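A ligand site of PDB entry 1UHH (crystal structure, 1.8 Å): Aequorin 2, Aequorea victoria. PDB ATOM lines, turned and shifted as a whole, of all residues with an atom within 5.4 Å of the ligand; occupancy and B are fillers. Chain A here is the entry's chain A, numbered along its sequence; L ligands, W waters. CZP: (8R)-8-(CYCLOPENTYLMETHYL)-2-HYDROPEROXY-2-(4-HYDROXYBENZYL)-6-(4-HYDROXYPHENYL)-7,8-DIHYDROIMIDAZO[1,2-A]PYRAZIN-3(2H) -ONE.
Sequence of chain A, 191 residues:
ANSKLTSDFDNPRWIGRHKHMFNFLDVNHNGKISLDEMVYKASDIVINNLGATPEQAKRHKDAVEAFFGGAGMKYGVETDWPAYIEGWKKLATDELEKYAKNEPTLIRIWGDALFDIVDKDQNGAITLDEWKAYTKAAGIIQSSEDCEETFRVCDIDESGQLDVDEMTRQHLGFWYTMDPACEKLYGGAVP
The side-chain hydroxyl (OH) of Tyr 84 sits at hydrogen-bond distance from an oxygen (O25) of the ligand.
A ring nitrogen (ND1) of His 18 is in hydrogen-bond range of an oxygen (O25) of the ligand (2.8 Å).
An oxygen (O32) of the ligand lies within hydrogen-bond range of the side-chain hydroxyl (OH) of Tyr 186, at 2.8 Å.
The side-chain hydroxyl (OH) of Tyr 134 sits at hydrogen-bond distance from a nitrogen (N1) of the ligand, 2.9 Å away.
An oxygen (O18) of the ligand lies close to a ring nitrogen (NE2) of His 171 (3.1 Å).
An oxygen (O18) of the ligand is in hydrogen-bond range of the indole nitrogen (NE1) of Trp 175.
NE1 of Trp 88 is in hydrogen-bond range of O25 of the ligand, 3.3 Å away.
OH of Tyr 84 sits at hydrogen-bond distance from NE1 of Trp 88 (3.1 Å).
NE2 of His 18 sits at hydrogen-bond distance from O of Trp 175, 3.0 Å away.
The side-chain hydroxyl (OH) of Tyr 186 is in hydrogen-bond range of a ring nitrogen (NE2) of His 171.
NZ of Lys 41 lies within hydrogen-bond range of O of Ala 138.
Met 21 touches the ligand.
Leu 25 touches the ligand.
Lys 41 touches the ligand (CE to C28, 3.9 Å).
CA of Ala 42 touches C29 of the ligand, 3.7 Å away.
CD1 of Ile 45 touches C28 of the ligand, at 3.8 Å.
Phe 68 touches the ligand.
Ile 107 touches the ligand.
Trp 110 touches the ligand.
CA of Gly 111 touches C13 of the ligand, at 3.6 Å.
Leu 114 touches the ligand (CD2 to C16, 3.6 Å).
Phe 115 touches the ligand (CE1 to C15, 3.8 Å).
CH2 of Trp 131 touches O32 of the ligand, at 3.9 Å.
CD1 of Ile 140 touches C8 of the ligand, 3.8 Å away.
Met 167 touches the ligand.
Hydrophobic or aromatic side chains that line the ligand: His 18, Met 21, Leu 25, Ala 42, Ile 45, Phe 68, Tyr 84, Trp 88, Ile 107, Trp 110, Leu 114, Phe 115, Trp 131, Tyr 134, Ile 140, Met 167, His 171, Trp 175 and Tyr 186.
Within 4 Å of the ligand: His 18, Met 21, Leu 25, Lys 41, Ala 42, Ile 45, Phe 68, Tyr 84, Trp 88, Ile 107, Trp 110, Gly 111, Leu 114, Phe 115, Trp 131, Tyr 134, Ile 140, Met 167, His 171, Trp 175 and Tyr 186.
Water W1 lies within hydrogen-bond range of an oxygen (O17) of the ligand (2.5 Å), the side-chain hydroxyl of Thr 168 (2.6 Å) and the backbone carbonyl oxygen of Ile 107 (3.0 Å).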
ATOM      1  N   HIS A  18     -12.432  -5.647  -8.476  1.00  0.00           N
ATOM      2  CA  HIS A  18     -13.311  -4.525  -8.798  1.00  0.00           C
ATOM      3  C   HIS A  18     -12.669  -3.441  -9.661  1.00  0.00           C
ATOM      4  O   HIS A  18     -13.362  -2.780 -10.403  1.00  0.00           O
ATOM      5  CB  HIS A  18     -13.933  -3.916  -7.534  1.00  0.00           C
ATOM      6  CG  HIS A  18     -14.914  -4.850  -6.913  1.00  0.00           C
ATOM      7  ND1 HIS A  18     -16.172  -5.066  -7.449  1.00  0.00           N
ATOM      8  CD2 HIS A  18     -14.783  -5.685  -5.858  1.00  0.00           C
ATOM      9  CE1 HIS A  18     -16.794  -5.972  -6.724  1.00  0.00           C
ATOM     10  NE2 HIS A  18     -15.971  -6.386  -5.763  1.00  0.00           N
ATOM     11  N   MET A  21     -13.260  -4.666 -13.138  1.00  0.00           N
ATOM     12  CA  MET A  21     -14.619  -4.370 -13.635  1.00  0.00           C
ATOM     13  C   MET A  21     -14.785  -2.886 -13.906  1.00  0.00           C
ATOM     14  O   MET A  21     -15.439  -2.469 -14.865  1.00  0.00           O
ATOM     15  CB  MET A  21     -15.646  -4.826 -12.618  1.00  0.00           C
ATOM     16  CG  MET A  21     -15.817  -6.304 -12.513  1.00  0.00           C
ATOM     17  SD  MET A  21     -16.052  -7.224 -14.202  1.00  0.00           S
ATOM     18  CE  MET A  21     -17.610  -6.470 -14.730  1.00  0.00           C
ATOM     19  N   PHE A  22     -14.246  -2.035 -13.037  1.00  0.00           N
ATOM     20  CA  PHE A  22     -14.232  -0.586 -13.293  1.00  0.00           C
ATOM     21  C   PHE A  22     -13.637  -0.276 -14.662  1.00  0.00           C
ATOM     22  O   PHE A  22     -14.240   0.477 -15.451  1.00  0.00           O
ATOM     23  CB  PHE A  22     -13.545   0.183 -12.154  1.00  0.00           C
ATOM     24  CG  PHE A  22     -13.483   1.692 -12.355  1.00  0.00           C
ATOM     25  CD1 PHE A  22     -14.497   2.499 -11.892  1.00  0.00           C
ATOM     26  CD2 PHE A  22     -12.444   2.295 -13.103  1.00  0.00           C
ATOM     27  CE1 PHE A  22     -14.482   3.845 -12.075  1.00  0.00           C
ATOM     28  CE2 PHE A  22     -12.419   3.656 -13.269  1.00  0.00           C
ATOM     29  CZ  PHE A  22     -13.413   4.427 -12.754  1.00  0.00           C
ATOM     30  N   PHE A  24     -13.206  -2.295 -17.203  1.00  0.00           N
ATOM     31  CA  PHE A  24     -14.037  -2.917 -18.265  1.00  0.00           C
ATOM     32  C   PHE A  24     -15.291  -2.071 -18.510  1.00  0.00           C
ATOM     33  O   PHE A  24     -15.755  -1.968 -19.682  1.00  0.00           O
ATOM     34  CB  PHE A  24     -14.403  -4.357 -17.893  1.00  0.00           C
ATOM     35  CG  PHE A  24     -15.694  -4.844 -18.525  1.00  0.00           C
ATOM     36  CD1 PHE A  24     -15.715  -5.251 -19.813  1.00  0.00           C
ATOM     37  CD2 PHE A  24     -16.844  -4.949 -17.786  1.00  0.00           C
ATOM     38  CE1 PHE A  24     -16.888  -5.670 -20.401  1.00  0.00           C
ATOM     39  CE2 PHE A  24     -18.016  -5.406 -18.361  1.00  0.00           C
ATOM     40  CZ  PHE A  24     -18.018  -5.777 -19.671  1.00  0.00           C
ATOM     41  N   LEU A  25     -15.880  -1.482 -17.449  1.00  0.00           N
ATOM     42  CA  LEU A  25     -17.085  -0.649 -17.605  1.00  0.00           C
ATOM     43  C   LEU A  25     -16.744   0.732 -18.168  1.00  0.00           C
ATOM     44  O   LEU A  25     -17.566   1.316 -18.847  1.00  0.00           O
ATOM     45  CB  LEU A  25     -17.819  -0.506 -16.252  1.00  0.00           C
ATOM     46  CG  LEU A  25     -18.420  -1.815 -15.748  1.00  0.00           C
ATOM     47  CD1 LEU A  25     -18.834  -1.730 -14.329  1.00  0.00           C
ATOM     48  CD2 LEU A  25     -19.599  -2.231 -16.599  1.00  0.00           C
ATOM     49  N   MET A  38     -24.270   2.969 -17.042  1.00  0.00           N
ATOM     50  CA  MET A  38     -24.500   1.614 -16.569  1.00  0.00           C
ATOM     51  C   MET A  38     -25.894   1.098 -16.953  1.00  0.00           C
ATOM     52  O   MET A  38     -26.023  -0.060 -17.375  1.00  0.00           O
ATOM     53  CB  MET A  38     -24.321   1.488 -15.050  1.00  0.00           C
ATOM     54  CG  MET A  38     -22.969   1.978 -14.512  1.00  0.00           C
ATOM     55  SD  MET A  38     -21.535   0.876 -15.210  1.00  0.00           S
ATOM     56  CE  MET A  38     -20.945   2.083 -16.792  1.00  0.00           C
ATOM     57  N   LYS A  41     -26.211   0.443 -20.766  1.00  0.00           N
ATOM     58  CA  LYS A  41     -25.549  -0.783 -21.181  1.00  0.00           C
ATOM     59  C   LYS A  41     -26.441  -1.959 -20.808  1.00  0.00           C
ATOM     60  O   LYS A  41     -26.661  -2.827 -21.613  1.00  0.00           O
ATOM     61  CB  LYS A  41     -24.167  -0.939 -20.465  1.00  0.00           C
ATOM     62  CG  LYS A  41     -23.404  -2.279 -20.779  1.00  0.00           C
ATOM     63  CD  LYS A  41     -22.133  -2.462 -19.942  1.00  0.00           C
ATOM     64  CE  LYS A  41     -21.401  -3.785 -20.199  1.00  0.00           C
ATOM     65  NZ  LYS A  41     -20.551  -3.801 -21.484  1.00  0.00           N
ATOM     66  N   ALA A  42     -26.971  -1.945 -19.578  1.00  0.00           N
ATOM     67  CA  ALA A  42     -27.786  -3.043 -19.092  1.00  0.00           C
ATOM     68  C   ALA A  42     -29.038  -3.273 -19.980  1.00  0.00           C
ATOM     69  O   ALA A  42     -29.359  -4.430 -20.322  1.00  0.00           O
ATOM     70  CB  ALA A  42     -28.204  -2.769 -17.668  1.00  0.00           C
ATOM     71  N   ILE A  45     -28.245  -4.499 -23.666  1.00  0.00           N
ATOM     72  CA  ILE A  45     -28.015  -5.952 -23.707  1.00  0.00           C
ATOM     73  C   ILE A  45     -29.340  -6.669 -23.725  1.00  0.00           C
ATOM     74  O   ILE A  45     -29.580  -7.485 -24.599  1.00  0.00           O
ATOM     75  CB  ILE A  45     -27.163  -6.456 -22.498  1.00  0.00           C
ATOM     76  CG1 ILE A  45     -25.710  -5.977 -22.613  1.00  0.00           C
ATOM     77  CG2 ILE A  45     -27.154  -7.935 -22.409  1.00  0.00           C
ATOM     78  CD1 ILE A  45     -24.973  -5.850 -21.286  1.00  0.00           C
ATOM     79  N   VAL A  64     -30.668  -3.189 -11.764  1.00  0.00           N
ATOM     80  CA  VAL A  64     -29.324  -2.625 -12.076  1.00  0.00           C
ATOM     81  C   VAL A  64     -29.122  -1.250 -11.458  1.00  0.00           C
ATOM     82  O   VAL A  64     -28.086  -1.012 -10.839  1.00  0.00           O
ATOM     83  CB  VAL A  64     -29.051  -2.590 -13.608  1.00  0.00           C
ATOM     84  CG1 VAL A  64     -27.762  -1.810 -13.893  1.00  0.00           C
ATOM     85  CG2 VAL A  64     -28.963  -4.031 -14.147  1.00  0.00           C
ATOM     86  N   PHE A  67     -28.639  -1.760  -7.733  1.00  0.00           N
ATOM     87  CA  PHE A  67     -27.290  -2.380  -7.503  1.00  0.00           C
ATOM     88  C   PHE A  67     -26.181  -1.322  -7.521  1.00  0.00           C
ATOM     89  O   PHE A  67     -25.480  -1.115  -6.544  1.00  0.00           O
ATOM     90  CB  PHE A  67     -27.020  -3.511  -8.541  1.00  0.00           C
ATOM     91  CG  PHE A  67     -25.718  -4.199  -8.395  1.00  0.00           C
ATOM     92  CD1 PHE A  67     -25.561  -5.226  -7.490  1.00  0.00           C
ATOM     93  CD2 PHE A  67     -24.642  -3.850  -9.222  1.00  0.00           C
ATOM     94  CE1 PHE A  67     -24.319  -5.887  -7.354  1.00  0.00           C
ATOM     95  CE2 PHE A  67     -23.419  -4.511  -9.118  1.00  0.00           C
ATOM     96  CZ  PHE A  67     -23.253  -5.533  -8.162  1.00  0.00           C
ATOM     97  N   PHE A  68     -25.976  -0.674  -8.657  1.00  0.00           N
ATOM     98  CA  PHE A  68     -24.986   0.361  -8.713  1.00  0.00           C
ATOM     99  C   PHE A  68     -25.325   1.562  -7.781  1.00  0.00           C
ATOM    100  O   PHE A  68     -24.426   2.215  -7.303  1.00  0.00           O
ATOM    101  CB  PHE A  68     -24.772   0.788 -10.158  1.00  0.00           C
ATOM    102  CG  PHE A  68     -24.018  -0.246 -11.006  1.00  0.00           C
ATOM    103  CD1 PHE A  68     -24.668  -0.948 -11.997  1.00  0.00           C
ATOM    104  CD2 PHE A  68     -22.636  -0.455 -10.838  1.00  0.00           C
ATOM    105  CE1 PHE A  68     -23.977  -1.849 -12.783  1.00  0.00           C
ATOM    106  CE2 PHE A  68     -21.955  -1.370 -11.568  1.00  0.00           C
ATOM    107  CZ  PHE A  68     -22.626  -2.063 -12.562  1.00  0.00           C
ATOM    108  N   TYR A  84     -15.653   4.963  -6.438  1.00  0.00           N
ATOM    109  CA  TYR A  84     -16.231   3.689  -6.844  1.00  0.00           C
ATOM    110  C   TYR A  84     -15.875   2.628  -5.820  1.00  0.00           C
ATOM    111  O   TYR A  84     -16.759   1.930  -5.290  1.00  0.00           O
ATOM    112  CB  TYR A  84     -15.721   3.305  -8.253  1.00  0.00           C
ATOM    113  CG  TYR A  84     -16.297   2.069  -8.807  1.00  0.00           C
ATOM    114  CD1 TYR A  84     -17.568   2.085  -9.405  1.00  0.00           C
ATOM    115  CD2 TYR A  84     -15.602   0.833  -8.747  1.00  0.00           C
ATOM    116  CE1 TYR A  84     -18.097   0.967  -9.952  1.00  0.00           C
ATOM    117  CE2 TYR A  84     -16.140  -0.308  -9.298  1.00  0.00           C
ATOM    118  CZ  TYR A  84     -17.393  -0.250  -9.897  1.00  0.00           C
ATOM    119  OH  TYR A  84     -17.941  -1.398 -10.404  1.00  0.00           O
ATOM    120  N   TRP A  88     -18.275   0.616  -3.224  1.00  0.00           N
ATOM    121  CA  TRP A  88     -18.334  -0.810  -3.300  1.00  0.00           C
ATOM    122  C   TRP A  88     -18.191  -1.478  -1.941  1.00  0.00           C
ATOM    123  O   TRP A  88     -18.845  -2.504  -1.671  1.00  0.00           O
ATOM    124  CB  TRP A  88     -17.336  -1.380  -4.317  1.00  0.00           C
ATOM    125  CG  TRP A  88     -18.078  -1.876  -5.520  1.00  0.00           C
ATOM    126  CD1 TRP A  88     -18.303  -1.195  -6.697  1.00  0.00           C
ATOM    127  CD2 TRP A  88     -18.750  -3.131  -5.652  1.00  0.00           C
ATOM    128  NE1 TRP A  88     -19.034  -1.979  -7.540  1.00  0.00           N
ATOM    129  CE2 TRP A  88     -19.340  -3.167  -6.930  1.00  0.00           C
ATOM    130  CE3 TRP A  88     -18.910  -4.252  -4.798  1.00  0.00           C
ATOM    131  CZ2 TRP A  88     -20.061  -4.250  -7.387  1.00  0.00           C
ATOM    132  CZ3 TRP A  88     -19.591  -5.337  -5.264  1.00  0.00           C
ATOM    133  CH2 TRP A  88     -20.161  -5.357  -6.558  1.00  0.00           C
ATOM    134  N   ILE A 107     -28.181  -8.337  -5.326  1.00  0.00           N
ATOM    135  CA  ILE A 107     -27.706  -9.304  -6.316  1.00  0.00           C
ATOM    136  C   ILE A 107     -28.719 -10.429  -6.620  1.00  0.00           C
ATOM    137  O   ILE A 107     -28.813 -10.841  -7.752  1.00  0.00           O
ATOM    138  CB  ILE A 107     -26.291  -9.821  -5.927  1.00  0.00           C
ATOM    139  CG1 ILE A 107     -25.716 -10.627  -7.080  1.00  0.00           C
ATOM    140  CG2 ILE A 107     -26.315 -10.582  -4.658  1.00  0.00           C
ATOM    141  CD1 ILE A 107     -25.474  -9.803  -8.290  1.00  0.00           C
ATOM    142  N   TRP A 110     -31.559  -8.797  -8.826  1.00  0.00           N
ATOM    143  CA  TRP A 110     -31.040  -8.653 -10.188  1.00  0.00           C
ATOM    144  C   TRP A 110     -30.982  -9.991 -10.864  1.00  0.00           C
ATOM    145  O   TRP A 110     -31.412 -10.151 -11.975  1.00  0.00           O
ATOM    146  CB  TRP A 110     -29.634  -8.009 -10.104  1.00  0.00           C
ATOM    147  CG  TRP A 110     -28.979  -7.740 -11.439  1.00  0.00           C
ATOM    148  CD1 TRP A 110     -29.548  -7.800 -12.730  1.00  0.00           C
ATOM    149  CD2 TRP A 110     -27.623  -7.365 -11.650  1.00  0.00           C
ATOM    150  NE1 TRP A 110     -28.590  -7.470 -13.679  1.00  0.00           N
ATOM    151  CE2 TRP A 110     -27.404  -7.229 -13.057  1.00  0.00           C
ATOM    152  CE3 TRP A 110     -26.540  -7.162 -10.809  1.00  0.00           C
ATOM    153  CZ2 TRP A 110     -26.182  -6.913 -13.588  1.00  0.00           C
ATOM    154  CZ3 TRP A 110     -25.337  -6.849 -11.350  1.00  0.00           C
ATOM    155  CH2 TRP A 110     -25.159  -6.738 -12.699  1.00  0.00           C
ATOM    156  N   GLY A 111     -30.392 -11.010 -10.193  1.00  0.00           N
ATOM    157  CA  GLY A 111     -30.376 -12.325 -10.762  1.00  0.00           C
ATOM    158  C   GLY A 111     -31.760 -12.825 -11.162  1.00  0.00           C
ATOM    159  O   GLY A 111     -31.952 -13.351 -12.249  1.00  0.00           O
ATOM    160  N   LEU A 114     -32.778 -11.006 -14.348  1.00  0.00           N
ATOM    161  CA  LEU A 114     -31.981 -11.412 -15.503  1.00  0.00           C
ATOM    162  C   LEU A 114     -32.356 -12.815 -15.928  1.00  0.00           C
ATOM    163  O   LEU A 114     -32.532 -13.085 -17.105  1.00  0.00           O
ATOM    164  CB  LEU A 114     -30.477 -11.305 -15.231  1.00  0.00           C
ATOM    165  CG  LEU A 114     -29.542 -11.615 -16.424  1.00  0.00           C
ATOM    166  CD1 LEU A 114     -29.822 -10.732 -17.622  1.00  0.00           C
ATOM    167  CD2 LEU A 114     -28.090 -11.492 -16.032  1.00  0.00           C
ATOM    168  N   PHE A 115     -32.492 -13.745 -14.965  1.00  0.00           N
ATOM    169  CA  PHE A 115     -32.828 -15.110 -15.338  1.00  0.00           C
ATOM    170  C   PHE A 115     -34.196 -15.217 -16.026  1.00  0.00           C
ATOM    171  O   PHE A 115     -34.365 -16.084 -16.862  1.00  0.00           O
ATOM    172  CB  PHE A 115     -32.779 -16.030 -14.113  1.00  0.00           C
ATOM    173  CG  PHE A 115     -31.429 -16.643 -13.863  1.00  0.00           C
ATOM    174  CD1 PHE A 115     -30.275 -15.857 -13.849  1.00  0.00           C
ATOM    175  CD2 PHE A 115     -31.294 -18.005 -13.672  1.00  0.00           C
ATOM    176  CE1 PHE A 115     -29.027 -16.429 -13.594  1.00  0.00           C
ATOM    177  CE2 PHE A 115     -30.016 -18.573 -13.407  1.00  0.00           C
ATOM    178  CZ  PHE A 115     -28.912 -17.804 -13.378  1.00  0.00           C
ATOM    179  N   TRP A 131     -25.841 -18.924 -20.920  1.00  0.00           N
ATOM    180  CA  TRP A 131     -24.797 -18.191 -20.222  1.00  0.00           C
ATOM    181  C   TRP A 131     -23.815 -17.557 -21.170  1.00  0.00           C
ATOM    182  O   TRP A 131     -23.401 -16.433 -20.941  1.00  0.00           O
ATOM    183  CB  TRP A 131     -24.063 -19.097 -19.227  1.00  0.00           C
ATOM    184  CG  TRP A 131     -22.968 -18.502 -18.402  1.00  0.00           C
ATOM    185  CD1 TRP A 131     -21.699 -18.945 -18.343  1.00  0.00           C
ATOM    186  CD2 TRP A 131     -23.045 -17.383 -17.481  1.00  0.00           C
ATOM    187  NE1 TRP A 131     -20.988 -18.196 -17.438  1.00  0.00           N
ATOM    188  CE2 TRP A 131     -21.787 -17.254 -16.887  1.00  0.00           C
ATOM    189  CE3 TRP A 131     -24.049 -16.522 -17.077  1.00  0.00           C
ATOM    190  CZ2 TRP A 131     -21.492 -16.241 -15.957  1.00  0.00           C
ATOM    191  CZ3 TRP A 131     -23.745 -15.519 -16.113  1.00  0.00           C
ATOM    192  CH2 TRP A 131     -22.495 -15.407 -15.575  1.00  0.00           C
ATOM    193  N   TYR A 134     -25.545 -14.375 -22.813  1.00  0.00           N
ATOM    194  CA  TYR A 134     -25.523 -13.183 -21.933  1.00  0.00           C
ATOM    195  C   TYR A 134     -24.107 -12.610 -21.775  1.00  0.00           C
ATOM    196  O   TYR A 134     -23.858 -11.403 -22.015  1.00  0.00           O
ATOM    197  CB  TYR A 134     -26.108 -13.496 -20.573  1.00  0.00           C
ATOM    198  CG  TYR A 134     -25.825 -12.390 -19.610  1.00  0.00           C
ATOM    199  CD1 TYR A 134     -26.459 -11.163 -19.739  1.00  0.00           C
ATOM    200  CD2 TYR A 134     -24.888 -12.526 -18.605  1.00  0.00           C
ATOM    201  CE1 TYR A 134     -26.163 -10.087 -18.943  1.00  0.00           C
ATOM    202  CE2 TYR A 134     -24.564 -11.409 -17.780  1.00  0.00           C
ATOM    203  CZ  TYR A 134     -25.195 -10.222 -17.970  1.00  0.00           C
ATOM    204  OH  TYR A 134     -24.959  -9.167 -17.170  1.00  0.00           O
ATOM    205  N   ALA A 138     -22.743  -8.914 -23.027  1.00  0.00           N
ATOM    206  CA  ALA A 138     -22.257  -7.949 -22.057  1.00  0.00           C
ATOM    207  C   ALA A 138     -20.750  -7.646 -22.274  1.00  0.00           C
ATOM    208  O   ALA A 138     -20.286  -6.531 -22.073  1.00  0.00           O
ATOM    209  CB  ALA A 138     -22.579  -8.457 -20.632  1.00  0.00           C
ATOM    210  N   ILE A 140     -18.461  -9.345 -20.531  1.00  0.00           N
ATOM    211  CA  ILE A 140     -17.763  -9.701 -19.276  1.00  0.00           C
ATOM    212  C   ILE A 140     -16.945 -11.004 -19.370  1.00  0.00           C
ATOM    213  O   ILE A 140     -15.892 -11.166 -18.691  1.00  0.00           O
ATOM    214  CB  ILE A 140     -18.771  -9.776 -18.072  1.00  0.00           C
ATOM    215  CG1 ILE A 140     -18.069  -9.913 -16.717  1.00  0.00           C
ATOM    216  CG2 ILE A 140     -19.745 -10.899 -18.239  1.00  0.00           C
ATOM    217  CD1 ILE A 140     -19.042  -9.654 -15.551  1.00  0.00           C
ATOM    218  N   VAL A 164     -30.524 -20.071 -10.290  1.00  0.00           N
ATOM    219  CA  VAL A 164     -30.320 -18.771  -9.680  1.00  0.00           C
ATOM    220  C   VAL A 164     -29.921 -18.858  -8.211  1.00  0.00           C
ATOM    221  O   VAL A 164     -29.135 -18.058  -7.728  1.00  0.00           O
ATOM    222  CB  VAL A 164     -31.586 -17.873  -9.858  1.00  0.00           C
ATOM    223  CG1 VAL A 164     -32.777 -18.434  -9.105  1.00  0.00           C
ATOM    224  CG2 VAL A 164     -31.303 -16.429  -9.396  1.00  0.00           C
ATOM    225  N   MET A 167     -26.152 -19.580  -8.441  1.00  0.00           N
ATOM    226  CA  MET A 167     -25.417 -18.416  -8.981  1.00  0.00           C
ATOM    227  C   MET A 167     -25.426 -17.264  -7.954  1.00  0.00           C
ATOM    228  O   MET A 167     -24.431 -16.600  -7.854  1.00  0.00           O
ATOM    229  CB  MET A 167     -25.975 -17.965 -10.377  1.00  0.00           C
ATOM    230  CG  MET A 167     -25.092 -16.973 -11.175  1.00  0.00           C
ATOM    231  SD  MET A 167     -23.150 -17.592 -11.078  1.00  0.00           S
ATOM    232  CE  MET A 167     -22.477 -16.872 -12.854  1.00  0.00           C
ATOM    233  N   THR A 168     -26.514 -17.046  -7.155  1.00  0.00           N
ATOM    234  CA  THR A 168     -26.531 -16.010  -6.135  1.00  0.00           C
ATOM    235  C   THR A 168     -25.472 -16.269  -5.059  1.00  0.00           C
ATOM    236  O   THR A 168     -24.705 -15.398  -4.682  1.00  0.00           O
ATOM    237  CB  THR A 168     -27.934 -15.906  -5.486  1.00  0.00           C
ATOM    238  OG1 THR A 168     -28.916 -15.549  -6.485  1.00  0.00           O
ATOM    239  CG2 THR A 168     -27.962 -14.813  -4.483  1.00  0.00           C
ATOM    240  N   HIS A 171     -22.041 -15.609  -6.557  1.00  0.00           N
ATOM    241  CA  HIS A 171     -21.788 -14.183  -6.697  1.00  0.00           C
ATOM    242  C   HIS A 171     -21.563 -13.466  -5.364  1.00  0.00           C
ATOM    243  O   HIS A 171     -20.743 -12.559  -5.279  1.00  0.00           O
ATOM    244  CB  HIS A 171     -22.989 -13.610  -7.391  1.00  0.00           C
ATOM    245  CG  HIS A 171     -22.876 -13.649  -8.852  1.00  0.00           C
ATOM    246  ND1 HIS A 171     -23.948 -13.437  -9.673  1.00  0.00           N
ATOM    247  CD2 HIS A 171     -21.799 -13.826  -9.653  1.00  0.00           C
ATOM    248  CE1 HIS A 171     -23.547 -13.513 -10.928  1.00  0.00           C
ATOM    249  NE2 HIS A 171     -22.251 -13.729 -10.948  1.00  0.00           N
ATOM    250  N   TRP A 175     -18.038 -11.588  -5.529  1.00  0.00           N
ATOM    251  CA  TRP A 175     -17.997 -10.134  -5.598  1.00  0.00           C
ATOM    252  C   TRP A 175     -17.852  -9.483  -4.204  1.00  0.00           C
ATOM    253  O   TRP A 175     -17.315  -8.439  -4.105  1.00  0.00           O
ATOM    254  CB  TRP A 175     -19.258  -9.584  -6.297  1.00  0.00           C
ATOM    255  CG  TRP A 175     -19.467 -10.000  -7.743  1.00  0.00           C
ATOM    256  CD1 TRP A 175     -20.629 -10.503  -8.262  1.00  0.00           C
ATOM    257  CD2 TRP A 175     -18.593  -9.807  -8.861  1.00  0.00           C
ATOM    258  NE1 TRP A 175     -20.493 -10.725  -9.604  1.00  0.00           N
ATOM    259  CE2 TRP A 175     -19.266 -10.275 -10.008  1.00  0.00           C
ATOM    260  CE3 TRP A 175     -17.311  -9.302  -9.019  1.00  0.00           C
ATOM    261  CZ2 TRP A 175     -18.686 -10.275 -11.262  1.00  0.00           C
ATOM    262  CZ3 TRP A 175     -16.761  -9.274 -10.282  1.00  0.00           C
ATOM    263  CH2 TRP A 175     -17.435  -9.753 -11.363  1.00  0.00           C
ATOM    264  N   TYR A 186     -15.628 -16.808 -13.405  1.00  0.00           N
ATOM    265  CA  TYR A 186     -15.708 -16.259 -14.778  1.00  0.00           C
ATOM    266  C   TYR A 186     -14.516 -16.715 -15.575  1.00  0.00           C
ATOM    267  O   TYR A 186     -14.113 -16.096 -16.541  1.00  0.00           O
ATOM    268  CB  TYR A 186     -15.780 -14.695 -14.758  1.00  0.00           C
ATOM    269  CG  TYR A 186     -17.109 -14.142 -14.287  1.00  0.00           C
ATOM    270  CD1 TYR A 186     -17.432 -14.073 -12.924  1.00  0.00           C
ATOM    271  CD2 TYR A 186     -18.044 -13.706 -15.205  1.00  0.00           C
ATOM    272  CE1 TYR A 186     -18.679 -13.580 -12.517  1.00  0.00           C
ATOM    273  CE2 TYR A 186     -19.292 -13.189 -14.785  1.00  0.00           C
ATOM    274  CZ  TYR A 186     -19.583 -13.162 -13.460  1.00  0.00           C
ATOM    275  OH  TYR A 186     -20.790 -12.678 -13.049  1.00  0.00           O
HETATM  276  O25 CZP L   1     -17.373  -3.853  -9.637  1.00  0.00           O
HETATM  277  C22 CZP L   1     -18.236  -4.672 -10.315  1.00  0.00           C
HETATM  278  C23 CZP L   1     -18.745  -4.278 -11.525  1.00  0.00           C
HETATM  279  C24 CZP L   1     -19.578  -5.079 -12.249  1.00  0.00           C
HETATM  280  C21 CZP L   1     -18.689  -5.870  -9.800  1.00  0.00           C
HETATM  281  C20 CZP L   1     -19.562  -6.672 -10.525  1.00  0.00           C
HETATM  282  C19 CZP L   1     -20.021  -6.283 -11.753  1.00  0.00           C
HETATM  283  C6  CZP L   1     -20.942  -7.105 -12.578  1.00  0.00           C
HETATM  284  N7  CZP L   1     -21.181  -6.672 -13.846  1.00  0.00           N
HETATM  285  C8  CZP L   1     -21.945  -7.320 -14.689  1.00  0.00           C
HETATM  286  C26 CZP L   1     -22.214  -6.774 -16.097  1.00  0.00           C
HETATM  287  C27 CZP L   1     -23.450  -5.949 -16.210  1.00  0.00           C
HETATM  288  C28 CZP L   1     -23.713  -5.661 -17.675  1.00  0.00           C
HETATM  289  C29 CZP L   1     -24.727  -4.532 -17.626  1.00  0.00           C
HETATM  290  C30 CZP L   1     -24.393  -3.755 -16.340  1.00  0.00           C
HETATM  291  C31 CZP L   1     -23.357  -4.586 -15.591  1.00  0.00           C
HETATM  292  C9  CZP L   1     -22.507  -8.562 -14.173  1.00  0.00           C
HETATM  293  N4  CZP L   1     -22.268  -8.982 -12.930  1.00  0.00           N
HETATM  294  C5  CZP L   1     -21.495  -8.280 -12.082  1.00  0.00           C
HETATM  295  N1  CZP L   1     -23.330  -9.393 -14.825  1.00  0.00           N
HETATM  296  C2  CZP L   1     -23.701 -10.516 -13.965  1.00  0.00           C
HETATM  297  C3  CZP L   1     -22.927 -10.152 -12.721  1.00  0.00           C
HETATM  298  O18 CZP L   1     -22.890 -10.811 -11.701  1.00  0.00           O
HETATM  299  O32 CZP L   1     -23.128 -11.769 -14.395  1.00  0.00           O
HETATM  300  C10 CZP L   1     -25.233 -10.460 -13.911  1.00  0.00           C
HETATM  301  C11 CZP L   1     -25.817 -11.498 -12.967  1.00  0.00           C
HETATM  302  C12 CZP L   1     -26.264 -11.135 -11.697  1.00  0.00           C
HETATM  303  C13 CZP L   1     -26.798 -12.115 -10.842  1.00  0.00           C
HETATM  304  C14 CZP L   1     -26.883 -13.457 -11.290  1.00  0.00           C
HETATM  305  O17 CZP L   1     -27.375 -14.448 -10.504  1.00  0.00           O
HETATM  306  C15 CZP L   1     -26.457 -13.789 -12.560  1.00  0.00           C
HETATM  307  C16 CZP L   1     -25.924 -12.796 -13.408  1.00  0.00           C
HETATM  308  O   HOH W   1     -28.195 -13.739  -8.260  1.00  0.00           O
